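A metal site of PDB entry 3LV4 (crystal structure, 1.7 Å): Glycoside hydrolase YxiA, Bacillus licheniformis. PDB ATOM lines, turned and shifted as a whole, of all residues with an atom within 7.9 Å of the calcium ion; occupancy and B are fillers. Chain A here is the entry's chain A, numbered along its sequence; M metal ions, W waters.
The backbone NH (N) of Asn 281 sits at hydrogen-bond distance from the side-chain hydroxyl (OG) of Ser 373, at 2.8 Å.
The side-chain carboxylate of Glu 358 sits at hydrogen-bond distance from the side-chain hydroxyl of Ser 373, at 2.6 Å.
Water W1 bridges OE1 of Glu 358 (2.8 Å) and O of Ser 373 (3.4 Å).
Within 4 Å of the calcium ion: Asn 281, Glu 358 and Glu 375.
The calcium ion is bound by OD1 of Asn 281, 2.4 Å away.
OE2 of Glu 358 binds the calcium ion (2.4 Å).
The side-chain carboxylate (OE2) of Glu 375 is bound to the calcium ion, 2.5 Å away.
Water W1 is bound to the calcium ion, 2.5 Å away.
Water W3 binds the calcium ion.
Water W2 is bound to the calcium ion, 2.8 Å away.
The calcium ion has six donor atoms within binding distance.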
ATOM      1  N   PHE A 280      -9.534  15.760  -7.342  1.00  0.00           N
ATOM      2  CA  PHE A 280      -8.631  15.203  -6.333  1.00  0.00           C
ATOM      3  C   PHE A 280      -8.442  13.718  -6.619  1.00  0.00           C
ATOM      4  O   PHE A 280      -9.401  12.946  -6.612  1.00  0.00           O
ATOM      5  CB  PHE A 280      -9.227  15.357  -4.938  1.00  0.00           C
ATOM      6  CG  PHE A 280      -9.058  16.735  -4.345  1.00  0.00           C
ATOM      7  CD1 PHE A 280      -7.812  17.173  -3.926  1.00  0.00           C
ATOM      8  CD2 PHE A 280     -10.160  17.563  -4.162  1.00  0.00           C
ATOM      9  CE1 PHE A 280      -7.655  18.428  -3.356  1.00  0.00           C
ATOM     10  CE2 PHE A 280     -10.012  18.832  -3.595  1.00  0.00           C
ATOM     11  CZ  PHE A 280      -8.746  19.262  -3.179  1.00  0.00           C
ATOM     12  N   ASN A 281      -7.199  13.324  -6.875  1.00  0.00           N
ATOM     13  CA  ASN A 281      -6.911  11.915  -7.137  1.00  0.00           C
ATOM     14  C   ASN A 281      -7.689  11.344  -8.309  1.00  0.00           C
ATOM     15  O   ASN A 281      -7.970  10.140  -8.354  1.00  0.00           O
ATOM     16  CB  ASN A 281      -7.167  11.084  -5.892  1.00  0.00           C
ATOM     17  CG  ASN A 281      -5.917  10.820  -5.132  1.00  0.00           C
ATOM     18  OD1 ASN A 281      -4.885  10.538  -5.738  1.00  0.00           O
ATOM     19  ND2 ASN A 281      -5.973  10.936  -3.813  1.00  0.00           N
ATOM     20  N   ASN A 282      -8.036  12.213  -9.256  1.00  0.00           N
ATOM     21  CA  ASN A 282      -8.821  11.800 -10.418  1.00  0.00           C
ATOM     22  C   ASN A 282     -10.137  11.135 -10.038  1.00  0.00           C
ATOM     23  O   ASN A 282     -10.699  10.377 -10.830  1.00  0.00           O
ATOM     24  CB  ASN A 282      -8.005  10.886 -11.336  1.00  0.00           C
ATOM     25  CG  ASN A 282      -8.661  10.694 -12.705  1.00  0.00           C
ATOM     26  OD1 ASN A 282      -9.133  11.656 -13.310  1.00  0.00           O
ATOM     27  ND2 ASN A 282      -8.708   9.445 -13.178  1.00  0.00           N
ATOM     28  N   LYS A 283     -10.628  11.411  -8.840  1.00  0.00           N
ATOM     29  CA  LYS A 283     -11.907  10.872  -8.406  1.00  0.00           C
ATOM     30  C   LYS A 283     -12.935  11.986  -8.371  1.00  0.00           C
ATOM     31  O   LYS A 283     -12.793  12.969  -7.634  1.00  0.00           O
ATOM     32  CB  LYS A 283     -11.798  10.180  -7.054  1.00  0.00           C
ATOM     33  CG  LYS A 283     -10.882   8.961  -7.111  1.00  0.00           C
ATOM     34  CD  LYS A 283     -10.572   8.393  -5.724  1.00  0.00           C
ATOM     35  CE  LYS A 283      -9.657   7.187  -5.861  1.00  0.00           C
ATOM     36  NZ  LYS A 283      -9.352   6.555  -4.539  1.00  0.00           N
ATOM     37  N   TYR A 357      -0.577  15.545   1.414  1.00  0.00           N
ATOM     38  CA  TYR A 357      -1.813  16.142   0.895  1.00  0.00           C
ATOM     39  C   TYR A 357      -1.890  15.997  -0.605  1.00  0.00           C
ATOM     40  O   TYR A 357      -0.863  15.956  -1.290  1.00  0.00           O
ATOM     41  CB  TYR A 357      -1.862  17.646   1.200  1.00  0.00           C
ATOM     42  CG  TYR A 357      -2.104  18.034   2.647  1.00  0.00           C
ATOM     43  CD1 TYR A 357      -3.351  18.487   3.053  1.00  0.00           C
ATOM     44  CD2 TYR A 357      -1.091  17.950   3.598  1.00  0.00           C
ATOM     45  CE1 TYR A 357      -3.582  18.854   4.382  1.00  0.00           C
ATOM     46  CE2 TYR A 357      -1.300  18.301   4.916  1.00  0.00           C
ATOM     47  CZ  TYR A 357      -2.555  18.759   5.300  1.00  0.00           C
ATOM     48  OH  TYR A 357      -2.783  19.116   6.608  1.00  0.00           O
ATOM     49  N   GLU A 358      -3.114  15.931  -1.124  1.00  0.00           N
ATOM     50  CA  GLU A 358      -3.350  16.202  -2.532  1.00  0.00           C
ATOM     51  C   GLU A 358      -3.452  17.713  -2.677  1.00  0.00           C
ATOM     52  O   GLU A 358      -4.214  18.353  -1.957  1.00  0.00           O
ATOM     53  CB  GLU A 358      -4.668  15.562  -2.993  1.00  0.00           C
ATOM     54  CG  GLU A 358      -4.645  14.063  -2.950  1.00  0.00           C
ATOM     55  CD  GLU A 358      -3.717  13.480  -3.989  1.00  0.00           C
ATOM     56  OE1 GLU A 358      -3.410  14.165  -4.997  1.00  0.00           O
ATOM     57  OE2 GLU A 358      -3.309  12.325  -3.790  1.00  0.00           O
ATOM     58  N   SER A 373      -5.040  16.832  -9.020  1.00  0.00           N
ATOM     59  CA  SER A 373      -4.277  17.081  -7.797  1.00  0.00           C
ATOM     60  C   SER A 373      -2.977  16.297  -7.844  1.00  0.00           C
ATOM     61  O   SER A 373      -2.901  15.232  -8.477  1.00  0.00           O
ATOM     62  CB  SER A 373      -5.073  16.707  -6.554  1.00  0.00           C
ATOM     63  OG  SER A 373      -5.235  15.293  -6.454  1.00  0.00           O
ATOM     64  N   LYS A 374      -1.957  16.823  -7.164  1.00  0.00           N
ATOM     65  CA  LYS A 374      -0.670  16.156  -7.055  1.00  0.00           C
ATOM     66  C   LYS A 374      -0.264  16.092  -5.588  1.00  0.00           C
ATOM     67  O   LYS A 374      -0.645  16.960  -4.792  1.00  0.00           O
ATOM     68  CB  LYS A 374       0.373  16.919  -7.868  1.00  0.00           C
ATOM     69  CG  LYS A 374      -0.021  17.047  -9.333  1.00  0.00           C
ATOM     70  CD  LYS A 374       1.139  17.420 -10.210  1.00  0.00           C
ATOM     71  CE  LYS A 374       0.727  17.350 -11.668  1.00  0.00           C
ATOM     72  NZ  LYS A 374       1.586  18.208 -12.518  1.00  0.00           N
ATOM     73  N   GLU A 375       0.505  15.068  -5.239  1.00  0.00           N
ATOM     74  CA  GLU A 375       0.883  14.848  -3.836  1.00  0.00           C
ATOM     75  C   GLU A 375       2.044  15.695  -3.359  1.00  0.00           C
ATOM     76  O   GLU A 375       3.074  15.805  -4.025  1.00  0.00           O
ATOM     77  CB  GLU A 375       1.196  13.367  -3.587  1.00  0.00           C
ATOM     78  CG  GLU A 375       0.047  12.460  -3.906  1.00  0.00           C
ATOM     79  CD  GLU A 375       0.291  11.032  -3.470  1.00  0.00           C
ATOM     80  OE1 GLU A 375       1.320  10.758  -2.810  1.00  0.00           O
ATOM     81  OE2 GLU A 375      -0.556  10.170  -3.777  1.00  0.00           O
ATOM     82  N   LEU A 443      -4.032  13.078   2.782  1.00  0.00           N
ATOM     83  CA  LEU A 443      -4.110  11.646   2.556  1.00  0.00           C
ATOM     84  C   LEU A 443      -4.527  10.908   3.816  1.00  0.00           C
ATOM     85  O   LEU A 443      -5.203   9.881   3.746  1.00  0.00           O
ATOM     86  CB  LEU A 443      -2.766  11.100   2.063  1.00  0.00           C
ATOM     87  CG  LEU A 443      -2.515  11.155   0.558  1.00  0.00           C
ATOM     88  CD1 LEU A 443      -2.601  12.574   0.046  1.00  0.00           C
ATOM     89  CD2 LEU A 443      -1.159  10.548   0.224  1.00  0.00           C
HETATM   90 CA    CA M   1      -2.598  10.412  -5.145  1.00  0.00          CA
HETATM   91  O   HOH W   1      -2.302  12.303  -6.762  1.00  0.00           O
HETATM   92  O   HOH W   2      -1.230   9.302  -7.344  1.00  0.00           O
HETATM   93  O   HOH W   3      -3.553   8.826  -3.203  1.00  0.00           O
